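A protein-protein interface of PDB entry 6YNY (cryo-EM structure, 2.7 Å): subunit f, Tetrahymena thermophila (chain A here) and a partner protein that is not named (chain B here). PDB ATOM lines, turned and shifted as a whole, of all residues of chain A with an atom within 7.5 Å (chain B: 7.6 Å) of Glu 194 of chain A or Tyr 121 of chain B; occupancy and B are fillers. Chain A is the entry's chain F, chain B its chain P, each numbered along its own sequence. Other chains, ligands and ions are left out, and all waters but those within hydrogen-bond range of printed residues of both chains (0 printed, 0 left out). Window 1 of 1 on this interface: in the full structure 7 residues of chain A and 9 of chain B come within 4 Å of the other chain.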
ATOM      1  N   CYS A 184       6.649  -7.366  32.338  1.00  0.00           N
ATOM      2  CA  CYS A 184       7.297  -6.368  31.499  1.00  0.00           C
ATOM      3  C   CYS A 184       8.254  -5.501  32.300  1.00  0.00           C
ATOM      4  O   CYS A 184       9.189  -4.929  31.730  1.00  0.00           O
ATOM      5  CB  CYS A 184       6.249  -5.491  30.821  1.00  0.00           C
ATOM      6  SG  CYS A 184       5.355  -6.280  29.469  1.00  0.00           S
ATOM      7  N   ARG A 185       8.039  -5.396  33.611  1.00  0.00           N
ATOM      8  CA  ARG A 185       8.973  -4.689  34.475  1.00  0.00           C
ATOM      9  C   ARG A 185      10.391  -5.207  34.294  1.00  0.00           C
ATOM     10  O   ARG A 185      11.355  -4.436  34.345  1.00  0.00           O
ATOM     11  CB  ARG A 185       8.517  -4.836  35.928  1.00  0.00           C
ATOM     12  CG  ARG A 185       9.417  -4.219  36.983  1.00  0.00           C
ATOM     13  CD  ARG A 185      10.588  -5.107  37.391  1.00  0.00           C
ATOM     14  NE  ARG A 185      10.222  -6.508  37.554  1.00  0.00           N
ATOM     15  CZ  ARG A 185       9.610  -7.006  38.621  1.00  0.00           C
ATOM     16  NH1 ARG A 185       9.284  -6.220  39.632  1.00  0.00           N
ATOM     17  NH2 ARG A 185       9.323  -8.295  38.675  1.00  0.00           N
ATOM     18  N   GLN A 187      11.853  -6.114  31.706  1.00  0.00           N
ATOM     19  CA  GLN A 187      12.481  -5.650  30.479  1.00  0.00           C
ATOM     20  C   GLN A 187      13.233  -4.342  30.660  1.00  0.00           C
ATOM     21  O   GLN A 187      13.989  -3.952  29.765  1.00  0.00           O
ATOM     22  CB  GLN A 187      11.429  -5.493  29.386  1.00  0.00           C
ATOM     23  CG  GLN A 187      10.590  -6.727  29.174  1.00  0.00           C
ATOM     24  CD  GLN A 187      11.422  -7.957  28.907  1.00  0.00           C
ATOM     25  OE1 GLN A 187      12.472  -7.888  28.271  1.00  0.00           O
ATOM     26  NE2 GLN A 187      10.965  -9.092  29.406  1.00  0.00           N
ATOM     27  N   ASN A 188      13.042  -3.655  31.783  1.00  0.00           N
ATOM     28  CA  ASN A 188      13.821  -2.463  32.074  1.00  0.00           C
ATOM     29  C   ASN A 188      15.255  -2.791  32.456  1.00  0.00           C
ATOM     30  O   ASN A 188      16.097  -1.889  32.470  1.00  0.00           O
ATOM     31  CB  ASN A 188      13.155  -1.667  33.190  1.00  0.00           C
ATOM     32  CG  ASN A 188      11.757  -1.235  32.835  1.00  0.00           C
ATOM     33  OD1 ASN A 188      11.425  -1.060  31.665  1.00  0.00           O
ATOM     34  ND2 ASN A 188      10.926  -1.060  33.844  1.00  0.00           N
ATOM     35  N   TYR A 189      15.545  -4.052  32.773  1.00  0.00           N
ATOM     36  CA  TYR A 189      16.912  -4.466  33.039  1.00  0.00           C
ATOM     37  C   TYR A 189      17.774  -4.421  31.788  1.00  0.00           C
ATOM     38  O   TYR A 189      19.003  -4.433  31.895  1.00  0.00           O
ATOM     39  CB  TYR A 189      16.921  -5.871  33.634  1.00  0.00           C
ATOM     40  CG  TYR A 189      16.508  -5.914  35.080  1.00  0.00           C
ATOM     41  CD1 TYR A 189      15.174  -5.886  35.441  1.00  0.00           C
ATOM     42  CD2 TYR A 189      17.454  -5.983  36.085  1.00  0.00           C
ATOM     43  CE1 TYR A 189      14.797  -5.921  36.758  1.00  0.00           C
ATOM     44  CE2 TYR A 189      17.087  -6.018  37.405  1.00  0.00           C
ATOM     45  CZ  TYR A 189      15.757  -5.988  37.740  1.00  0.00           C
ATOM     46  OH  TYR A 189      15.389  -6.024  39.062  1.00  0.00           O
ATOM     47  N   ARG A 190      17.155  -4.375  30.610  1.00  0.00           N
ATOM     48  CA  ARG A 190      17.919  -4.220  29.379  1.00  0.00           C
ATOM     49  C   ARG A 190      18.729  -2.932  29.396  1.00  0.00           C
ATOM     50  O   ARG A 190      19.846  -2.885  28.870  1.00  0.00           O
ATOM     51  CB  ARG A 190      16.976  -4.240  28.182  1.00  0.00           C
ATOM     52  CG  ARG A 190      16.094  -5.465  28.108  1.00  0.00           C
ATOM     53  CD  ARG A 190      15.174  -5.408  26.914  1.00  0.00           C
ATOM     54  NE  ARG A 190      14.331  -6.590  26.809  1.00  0.00           N
ATOM     55  CZ  ARG A 190      13.701  -6.958  25.701  1.00  0.00           C
ATOM     56  NH1 ARG A 190      13.822  -6.249  24.594  1.00  0.00           N
ATOM     57  NH2 ARG A 190      12.954  -8.046  25.698  1.00  0.00           N
ATOM     58  N   LEU A 191      18.180  -1.877  29.997  1.00  0.00           N
ATOM     59  CA  LEU A 191      18.925  -0.633  30.141  1.00  0.00           C
ATOM     60  C   LEU A 191      20.218  -0.848  30.911  1.00  0.00           C
ATOM     61  O   LEU A 191      21.250  -0.252  30.586  1.00  0.00           O
ATOM     62  CB  LEU A 191      18.062   0.405  30.849  1.00  0.00           C
ATOM     63  CG  LEU A 191      16.779   0.822  30.145  1.00  0.00           C
ATOM     64  CD1 LEU A 191      15.849   1.505  31.116  1.00  0.00           C
ATOM     65  CD2 LEU A 191      17.101   1.740  28.998  1.00  0.00           C
ATOM     66  N   TYR A 192      20.180  -1.694  31.938  1.00  0.00           N
ATOM     67  CA  TYR A 192      21.368  -1.917  32.751  1.00  0.00           C
ATOM     68  C   TYR A 192      22.442  -2.651  31.963  1.00  0.00           C
ATOM     69  O   TYR A 192      23.625  -2.308  32.047  1.00  0.00           O
ATOM     70  CB  TYR A 192      20.997  -2.700  34.009  1.00  0.00           C
ATOM     71  CG  TYR A 192      19.854  -2.111  34.799  1.00  0.00           C
ATOM     72  CD1 TYR A 192      19.118  -2.891  35.672  1.00  0.00           C
ATOM     73  CD2 TYR A 192      19.512  -0.778  34.674  1.00  0.00           C
ATOM     74  CE1 TYR A 192      18.078  -2.362  36.393  1.00  0.00           C
ATOM     75  CE2 TYR A 192      18.471  -0.242  35.391  1.00  0.00           C
ATOM     76  CZ  TYR A 192      17.758  -1.037  36.248  1.00  0.00           C
ATOM     77  OH  TYR A 192      16.720  -0.500  36.968  1.00  0.00           O
ATOM     78  N   PHE A 193      22.049  -3.665  31.196  1.00  0.00           N
ATOM     79  CA  PHE A 193      23.014  -4.419  30.410  1.00  0.00           C
ATOM     80  C   PHE A 193      23.654  -3.559  29.333  1.00  0.00           C
ATOM     81  O   PHE A 193      24.822  -3.765  28.989  1.00  0.00           O
ATOM     82  CB  PHE A 193      22.334  -5.635  29.789  1.00  0.00           C
ATOM     83  CG  PHE A 193      21.645  -6.512  30.786  1.00  0.00           C
ATOM     84  CD1 PHE A 193      22.206  -6.749  32.023  1.00  0.00           C
ATOM     85  CD2 PHE A 193      20.429  -7.090  30.493  1.00  0.00           C
ATOM     86  CE1 PHE A 193      21.575  -7.548  32.937  1.00  0.00           C
ATOM     87  CE2 PHE A 193      19.794  -7.892  31.409  1.00  0.00           C
ATOM     88  CZ  PHE A 193      20.368  -8.120  32.631  1.00  0.00           C
ATOM     89  N   GLU A 194      22.912  -2.596  28.790  1.00  0.00           N
ATOM     90  CA  GLU A 194      23.460  -1.724  27.761  1.00  0.00           C
ATOM     91  C   GLU A 194      24.379  -0.664  28.353  1.00  0.00           C
ATOM     92  O   GLU A 194      25.381  -0.292  27.732  1.00  0.00           O
ATOM     93  CB  GLU A 194      22.322  -1.073  26.981  1.00  0.00           C
ATOM     94  CG  GLU A 194      21.439  -2.068  26.254  1.00  0.00           C
ATOM     95  CD  GLU A 194      20.183  -1.435  25.692  1.00  0.00           C
ATOM     96  OE1 GLU A 194      20.066  -0.193  25.737  1.00  0.00           O
ATOM     97  OE2 GLU A 194      19.307  -2.182  25.208  1.00  0.00           O
ATOM     98  N   MET A 195      24.056  -0.167  29.547  1.00  0.00           N
ATOM     99  CA  MET A 195      24.920   0.812  30.196  1.00  0.00           C
ATOM    100  C   MET A 195      26.237   0.183  30.623  1.00  0.00           C
ATOM    101  O   MET A 195      27.301   0.793  30.470  1.00  0.00           O
ATOM    102  CB  MET A 195      24.206   1.419  31.401  1.00  0.00           C
ATOM    103  CG  MET A 195      25.015   2.455  32.161  1.00  0.00           C
ATOM    104  SD  MET A 195      25.205   4.013  31.283  1.00  0.00           S
ATOM    105  CE  MET A 195      23.598   4.732  31.582  1.00  0.00           C
ATOM    106  N   ARG A 196      26.185  -1.035  31.160  1.00  0.00           N
ATOM    107  CA  ARG A 196      27.404  -1.703  31.599  1.00  0.00           C
ATOM    108  C   ARG A 196      28.392  -1.857  30.453  1.00  0.00           C
ATOM    109  O   ARG A 196      29.606  -1.750  30.653  1.00  0.00           O
ATOM    110  CB  ARG A 196      27.059  -3.063  32.197  1.00  0.00           C
ATOM    111  CG  ARG A 196      26.325  -2.970  33.510  1.00  0.00           C
ATOM    112  CD  ARG A 196      25.692  -4.284  33.902  1.00  0.00           C
ATOM    113  NE  ARG A 196      26.669  -5.358  34.044  1.00  0.00           N
ATOM    114  CZ  ARG A 196      27.372  -5.594  35.146  1.00  0.00           C
ATOM    115  NH1 ARG A 196      28.233  -6.597  35.173  1.00  0.00           N
ATOM    116  NH2 ARG A 196      27.226  -4.830  36.215  1.00  0.00           N
ATOM    117  N   LYS A 197      27.893  -2.110  29.245  1.00  0.00           N
ATOM    118  CA  LYS A 197      28.777  -2.243  28.096  1.00  0.00           C
ATOM    119  C   LYS A 197      29.292  -0.897  27.616  1.00  0.00           C
ATOM    120  O   LYS A 197      30.425  -0.810  27.131  1.00  0.00           O
ATOM    121  CB  LYS A 197      28.054  -2.960  26.959  1.00  0.00           C
ATOM    122  CG  LYS A 197      27.724  -4.396  27.264  1.00  0.00           C
ATOM    123  CD  LYS A 197      27.352  -5.153  26.016  1.00  0.00           C
ATOM    124  CE  LYS A 197      27.251  -6.633  26.294  1.00  0.00           C
ATOM    125  NZ  LYS A 197      27.018  -7.418  25.065  1.00  0.00           N
ATOM    126  N   LYS A 198      28.486   0.157  27.741  1.00  0.00           N
ATOM    127  CA  LYS A 198      28.940   1.479  27.330  1.00  0.00           C
ATOM    128  C   LYS A 198      30.044   1.986  28.248  1.00  0.00           C
ATOM    129  O   LYS A 198      31.020   2.584  27.784  1.00  0.00           O
ATOM    130  CB  LYS A 198      27.766   2.452  27.316  1.00  0.00           C
ATOM    131  CG  LYS A 198      28.110   3.820  26.782  1.00  0.00           C
ATOM    132  CD  LYS A 198      26.889   4.709  26.697  1.00  0.00           C
ATOM    133  CE  LYS A 198      26.429   5.145  28.070  1.00  0.00           C
ATOM    134  NZ  LYS A 198      25.258   6.049  27.991  1.00  0.00           N
ATOM    135  N   LEU A 199      29.907   1.757  29.551  1.00  0.00           N
ATOM    136  CA  LEU A 199      30.913   2.165  30.518  1.00  0.00           C
ATOM    137  C   LEU A 199      32.098   1.212  30.582  1.00  0.00           C
ATOM    138  O   LEU A 199      33.024   1.455  31.363  1.00  0.00           O
ATOM    139  CB  LEU A 199      30.282   2.282  31.904  1.00  0.00           C
ATOM    140  CG  LEU A 199      29.058   3.188  32.017  1.00  0.00           C
ATOM    141  CD1 LEU A 199      28.595   3.243  33.451  1.00  0.00           C
ATOM    142  CD2 LEU A 199      29.350   4.577  31.508  1.00  0.00           C
ATOM    143  N   GLY A 200      32.093   0.140  29.795  1.00  0.00           N
ATOM    144  CA  GLY A 200      33.194  -0.799  29.805  1.00  0.00           C
ATOM    145  C   GLY A 200      33.223  -1.718  31.001  1.00  0.00           C
ATOM    146  O   GLY A 200      34.306  -2.072  31.475  1.00  0.00           O
ATOM    147  N   PRO B 115      25.473  -7.066  20.029  1.00  0.00           N
ATOM    148  CA  PRO B 115      24.166  -7.035  20.682  1.00  0.00           C
ATOM    149  C   PRO B 115      23.205  -8.066  20.109  1.00  0.00           C
ATOM    150  O   PRO B 115      23.320  -8.506  18.964  1.00  0.00           O
ATOM    151  CB  PRO B 115      23.677  -5.614  20.381  1.00  0.00           C
ATOM    152  CG  PRO B 115      24.247  -5.325  19.056  1.00  0.00           C
ATOM    153  CD  PRO B 115      25.560  -6.055  18.964  1.00  0.00           C
ATOM    154  N   GLU B 116      22.245  -8.446  20.944  1.00  0.00           N
ATOM    155  CA  GLU B 116      21.144  -9.309  20.539  1.00  0.00           C
ATOM    156  C   GLU B 116      19.929  -8.419  20.323  1.00  0.00           C
ATOM    157  O   GLU B 116      19.416  -7.817  21.270  1.00  0.00           O
ATOM    158  CB  GLU B 116      20.874 -10.382  21.588  1.00  0.00           C
ATOM    159  CG  GLU B 116      22.072 -11.258  21.897  1.00  0.00           C
ATOM    160  CD  GLU B 116      21.791 -12.273  22.985  1.00  0.00           C
ATOM    161  OE1 GLU B 116      20.609 -12.623  23.184  1.00  0.00           O
ATOM    162  OE2 GLU B 116      22.751 -12.717  23.648  1.00  0.00           O
ATOM    163  N   LEU B 117      19.476  -8.334  19.073  1.00  0.00           N
ATOM    164  CA  LEU B 117      18.403  -7.410  18.733  1.00  0.00           C
ATOM    165  C   LEU B 117      17.158  -7.661  19.567  1.00  0.00           C
ATOM    166  O   LEU B 117      16.417  -6.722  19.878  1.00  0.00           O
ATOM    167  CB  LEU B 117      18.078  -7.530  17.249  1.00  0.00           C
ATOM    168  CG  LEU B 117      17.224  -6.426  16.640  1.00  0.00           C
ATOM    169  CD1 LEU B 117      17.982  -5.125  16.614  1.00  0.00           C
ATOM    170  CD2 LEU B 117      16.805  -6.813  15.255  1.00  0.00           C
ATOM    171  N   SER B 118      16.913  -8.913  19.939  1.00  0.00           N
ATOM    172  CA  SER B 118      15.764  -9.261  20.759  1.00  0.00           C
ATOM    173  C   SER B 118      15.938  -8.875  22.220  1.00  0.00           C
ATOM    174  O   SER B 118      14.958  -8.913  22.971  1.00  0.00           O
ATOM    175  CB  SER B 118      15.498 -10.761  20.659  1.00  0.00           C
ATOM    176  OG  SER B 118      14.390 -11.131  21.455  1.00  0.00           O
ATOM    177  N   LYS B 119      17.145  -8.502  22.636  1.00  0.00           N
ATOM    178  CA  LYS B 119      17.427  -8.154  24.020  1.00  0.00           C
ATOM    179  C   LYS B 119      17.591  -6.658  24.233  1.00  0.00           C
ATOM    180  O   LYS B 119      17.855  -6.232  25.361  1.00  0.00           O
ATOM    181  CB  LYS B 119      18.696  -8.869  24.492  1.00  0.00           C
ATOM    182  CG  LYS B 119      18.676 -10.367  24.328  1.00  0.00           C
ATOM    183  CD  LYS B 119      17.658 -11.011  25.225  1.00  0.00           C
ATOM    184  CE  LYS B 119      17.711 -12.516  25.109  1.00  0.00           C
ATOM    185  NZ  LYS B 119      19.038 -13.055  25.497  1.00  0.00           N
ATOM    186  N   LEU B 120      17.458  -5.852  23.186  1.00  0.00           N
ATOM    187  CA  LEU B 120      17.657  -4.417  23.307  1.00  0.00           C
ATOM    188  C   LEU B 120      16.395  -3.735  23.812  1.00  0.00           C
ATOM    189  O   LEU B 120      15.275  -4.203  23.591  1.00  0.00           O
ATOM    190  CB  LEU B 120      18.059  -3.814  21.963  1.00  0.00           C
ATOM    191  CG  LEU B 120      19.400  -4.255  21.382  1.00  0.00           C
ATOM    192  CD1 LEU B 120      19.625  -3.604  20.046  1.00  0.00           C
ATOM    193  CD2 LEU B 120      20.532  -3.918  22.316  1.00  0.00           C
ATOM    194  N   TYR B 121      16.591  -2.615  24.496  1.00  0.00           N
ATOM    195  CA  TYR B 121      15.489  -1.816  25.004  1.00  0.00           C
ATOM    196  C   TYR B 121      15.010  -0.859  23.925  1.00  0.00           C
ATOM    197  O   TYR B 121      15.814  -0.246  23.218  1.00  0.00           O
ATOM    198  CB  TYR B 121      15.919  -1.034  26.244  1.00  0.00           C
ATOM    199  CG  TYR B 121      14.805  -0.289  26.931  1.00  0.00           C
ATOM    200  CD1 TYR B 121      14.086  -0.872  27.963  1.00  0.00           C
ATOM    201  CD2 TYR B 121      14.476   1.001  26.557  1.00  0.00           C
ATOM    202  CE1 TYR B 121      13.072  -0.193  28.594  1.00  0.00           C
ATOM    203  CE2 TYR B 121      13.462   1.687  27.183  1.00  0.00           C
ATOM    204  CZ  TYR B 121      12.764   1.086  28.201  1.00  0.00           C
ATOM    205  OH  TYR B 121      11.753   1.768  28.831  1.00  0.00           O
ATOM    206  N   PHE B 122      13.693  -0.740  23.802  1.00  0.00           N
ATOM    207  CA  PHE B 122      13.098   0.144  22.818  1.00  0.00           C
ATOM    208  C   PHE B 122      11.781   0.666  23.363  1.00  0.00           C
ATOM    209  O   PHE B 122      11.254   0.171  24.361  1.00  0.00           O
ATOM    210  CB  PHE B 122      12.888  -0.560  21.479  1.00  0.00           C
ATOM    211  CG  PHE B 122      11.851  -1.640  21.514  1.00  0.00           C
ATOM    212  CD1 PHE B 122      10.540  -1.366  21.183  1.00  0.00           C
ATOM    213  CD2 PHE B 122      12.186  -2.930  21.865  1.00  0.00           C
ATOM    214  CE1 PHE B 122       9.591  -2.353  21.209  1.00  0.00           C
ATOM    215  CE2 PHE B 122      11.238  -3.916  21.891  1.00  0.00           C
ATOM    216  CZ  PHE B 122       9.940  -3.629  21.563  1.00  0.00           C
ATOM    217  N   PHE B 123      11.254   1.681  22.688  1.00  0.00           N
ATOM    218  CA  PHE B 123       9.998   2.295  23.075  1.00  0.00           C
ATOM    219  C   PHE B 123       9.216   2.634  21.818  1.00  0.00           C
ATOM    220  O   PHE B 123       9.761   2.675  20.714  1.00  0.00           O
ATOM    221  CB  PHE B 123      10.223   3.549  23.923  1.00  0.00           C
ATOM    222  CG  PHE B 123      10.493   4.783  23.124  1.00  0.00           C
ATOM    223  CD1 PHE B 123      11.570   4.847  22.264  1.00  0.00           C
ATOM    224  CD2 PHE B 123       9.675   5.887  23.242  1.00  0.00           C
ATOM    225  CE1 PHE B 123      11.816   5.981  21.533  1.00  0.00           C
ATOM    226  CE2 PHE B 123       9.919   7.022  22.515  1.00  0.00           C
ATOM    227  CZ  PHE B 123      10.991   7.070  21.659  1.00  0.00           C
ATOM    228  N   SER B 133      11.268   2.127  18.439  1.00  0.00           N
ATOM    229  CA  SER B 133      12.470   2.907  18.202  1.00  0.00           C
ATOM    230  C   SER B 133      13.514   2.592  19.259  1.00  0.00           C
ATOM    231  O   SER B 133      13.196   2.480  20.445  1.00  0.00           O
ATOM    232  CB  SER B 133      12.169   4.407  18.206  1.00  0.00           C
ATOM    233  OG  SER B 133      13.326   5.158  17.901  1.00  0.00           O
ATOM    234  N   LEU B 134      14.760   2.443  18.814  1.00  0.00           N
ATOM    235  CA  LEU B 134      15.875   2.276  19.732  1.00  0.00           C
ATOM    236  C   LEU B 134      16.333   3.593  20.333  1.00  0.00           C
ATOM    237  O   LEU B 134      16.988   3.589  21.379  1.00  0.00           O
ATOM    238  CB  LEU B 134      17.052   1.622  19.016  1.00  0.00           C
ATOM    239  CG  LEU B 134      16.823   0.218  18.471  1.00  0.00           C
ATOM    240  CD1 LEU B 134      18.048  -0.246  17.733  1.00  0.00           C
ATOM    241  CD2 LEU B 134      16.477  -0.740  19.587  1.00  0.00           C
ATOM    242  N   ASN B 135      16.005   4.716  19.697  1.00  0.00           N
ATOM    243  CA  ASN B 135      16.449   6.030  20.150  1.00  0.00           C
ATOM    244  C   ASN B 135      15.539   6.543  21.267  1.00  0.00           C
ATOM    245  O   ASN B 135      14.848   7.552  21.142  1.00  0.00           O
ATOM    246  CB  ASN B 135      16.486   6.997  18.977  1.00  0.00           C
ATOM    247  CG  ASN B 135      17.215   6.429  17.781  1.00  0.00           C
ATOM    248  OD1 ASN B 135      16.727   6.493  16.653  1.00  0.00           O
ATOM    249  ND2 ASN B 135      18.386   5.859  18.021  1.00  0.00           N
ATOM    250  N   HIS B 136      15.549   5.815  22.378  1.00  0.00           N
ATOM    251  CA  HIS B 136      14.748   6.209  23.521  1.00  0.00           C
ATOM    252  C   HIS B 136      15.405   7.374  24.254  1.00  0.00           C
ATOM    253  O   HIS B 136      16.577   7.698  24.050  1.00  0.00           O
ATOM    254  CB  HIS B 136      14.523   5.025  24.460  1.00  0.00           C
ATOM    255  CG  HIS B 136      15.780   4.344  24.894  1.00  0.00           C
ATOM    256  ND1 HIS B 136      16.523   4.770  25.972  1.00  0.00           N
ATOM    257  CD2 HIS B 136      16.421   3.261  24.399  1.00  0.00           C
ATOM    258  CE1 HIS B 136      17.571   3.980  26.120  1.00  0.00           C
ATOM    259  NE2 HIS B 136      17.533   3.057  25.177  1.00  0.00           N
ATOM    260  N   HIS B 137      14.624   8.006  25.124  1.00  0.00           N
ATOM    261  CA  HIS B 137      15.011   9.263  25.747  1.00  0.00           C
ATOM    262  C   HIS B 137      16.157   9.128  26.736  1.00  0.00           C
ATOM    263  O   HIS B 137      16.554  10.137  27.327  1.00  0.00           O
ATOM    264  CB  HIS B 137      13.793   9.878  26.427  1.00  0.00           C
ATOM    265  CG  HIS B 137      12.704  10.245  25.472  1.00  0.00           C
ATOM    266  ND1 HIS B 137      11.945   9.303  24.813  1.00  0.00           N
ATOM    267  CD2 HIS B 137      12.262  11.450  25.045  1.00  0.00           C
ATOM    268  CE1 HIS B 137      11.074   9.913  24.030  1.00  0.00           C
ATOM    269  NE2 HIS B 137      11.245  11.216  24.153  1.00  0.00           N
ATOM    270  N   ALA B 138      16.696   7.930  26.933  1.00  0.00           N
ATOM    271  CA  ALA B 138      17.890   7.732  27.740  1.00  0.00           C
ATOM    272  C   ALA B 138      19.136   7.507  26.897  1.00  0.00           C
ATOM    273  O   ALA B 138      20.215   7.288  27.454  1.00  0.00           O
ATOM    274  CB  ALA B 138      17.693   6.552  28.691  1.00  0.00           C
ATOM    275  N   VAL B 139      19.012   7.551  25.576  1.00  0.00           N
ATOM    276  CA  VAL B 139      20.149   7.379  24.682  1.00  0.00           C
ATOM    277  C   VAL B 139      20.954   8.668  24.631  1.00  0.00           C
ATOM    278  O   VAL B 139      20.414   9.773  24.752  1.00  0.00           O
ATOM    279  CB  VAL B 139      19.663   6.958  23.282  1.00  0.00           C
ATOM    280  CG1 VAL B 139      20.822   6.862  22.316  1.00  0.00           C
ATOM    281  CG2 VAL B 139      18.943   5.640  23.363  1.00  0.00           C
ATOM    282  N   ARG B 143      25.206   3.782  18.454  1.00  0.00           N
ATOM    283  CA  ARG B 143      25.650   2.392  18.496  1.00  0.00           C
ATOM    284  C   ARG B 143      27.062   2.223  17.944  1.00  0.00           C
ATOM    285  O   ARG B 143      27.941   1.688  18.625  1.00  0.00           O
ATOM    286  CB  ARG B 143      24.656   1.523  17.724  1.00  0.00           C
ATOM    287  CG  ARG B 143      23.214   1.694  18.184  1.00  0.00           C
ATOM    288  CD  ARG B 143      22.968   1.055  19.530  1.00  0.00           C
ATOM    289  NE  ARG B 143      21.666   1.427  20.071  1.00  0.00           N
ATOM    290  CZ  ARG B 143      21.132   0.903  21.169  1.00  0.00           C
ATOM    291  NH1 ARG B 143      21.783  -0.030  21.851  1.00  0.00           N
ATOM    292  NH2 ARG B 143      19.942   1.313  21.583  1.00  0.00           N
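Of the printed residues of chain B, Asn 188 of chain A touches Tyr 121 (3.6 Å).
Glu 194 of chain A touches two residues of chain B.
Printed residues of chain A within 4 Å of Ser 118 of chain B: Arg 190 (3.3 Å).
Tyr 121 of chain B touches just these residues of chain A: Gln 187, Asn 188, Arg 190, Leu 191 and Glu 194.
Of the printed residues of chain A, His 136 of chain B touches Leu 191.
The nearest residue of chain B that does not touch Glu 194 of chain A is His 136 of chain B (4.2 Å).
The nearest printed residue of chain A that does not touch Lys 119 of chain B is Glu 194 of chain A (4.3 Å).
Of the 16 printed residues of chain A, 5 touch a printed residue of chain B.
Of the 17 printed residues of chain B, 5 touch a printed residue of chain A.
Among the printed residues, 10 pairs touch across the chains.
Among the printed residues, no Asp or Glu carboxylate lies within 4 Å of a Lys or Arg side-chain nitrogen of the other chain.
NZ of Lys 119 of chain B is in salt-bridge range of OE1 of Glu 116 of chain B (2.8 Å).
N of Ala 138 of chain B sits close to ND1 of His 136 of chain B.
The side-chain amide nitrogen of Asn 188 of chain A sits at hydrogen-bond distance from the backbone carbonyl oxygen of Arg 185 of chain A.
NH2 of Arg 190 of chain A lies within hydrogen-bond range of OE1 of Gln 187 of chain A (2.6 Å).
O of Ser 118 of chain B sits at hydrogen-bond distance from NH1 of Arg 190 of chain A.
NH1 of Arg 190 of chain A is in hydrogen-bond range of O of Leu 120 of chain B (2.7 Å).
The backbone NH of Tyr 121 of chain B lies within hydrogen-bond range of the side-chain carboxylate of Glu 194 of chain A (2.8 Å).
Among the printed residues, merely in contact across the chains: Arg 190 of chain A with Lys 119 of chain B, Glu 194 of chain A with Leu 120 of chain B, Gln 187 of chain A with Tyr 121 of chain B, Asn 188 of chain A with Tyr 121 of chain B, Leu 191 of chain A with Tyr 121 of chain B, Leu 191 of chain A with His 136 of chain B and Arg 190 of chain A with Tyr 121 of chain B.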
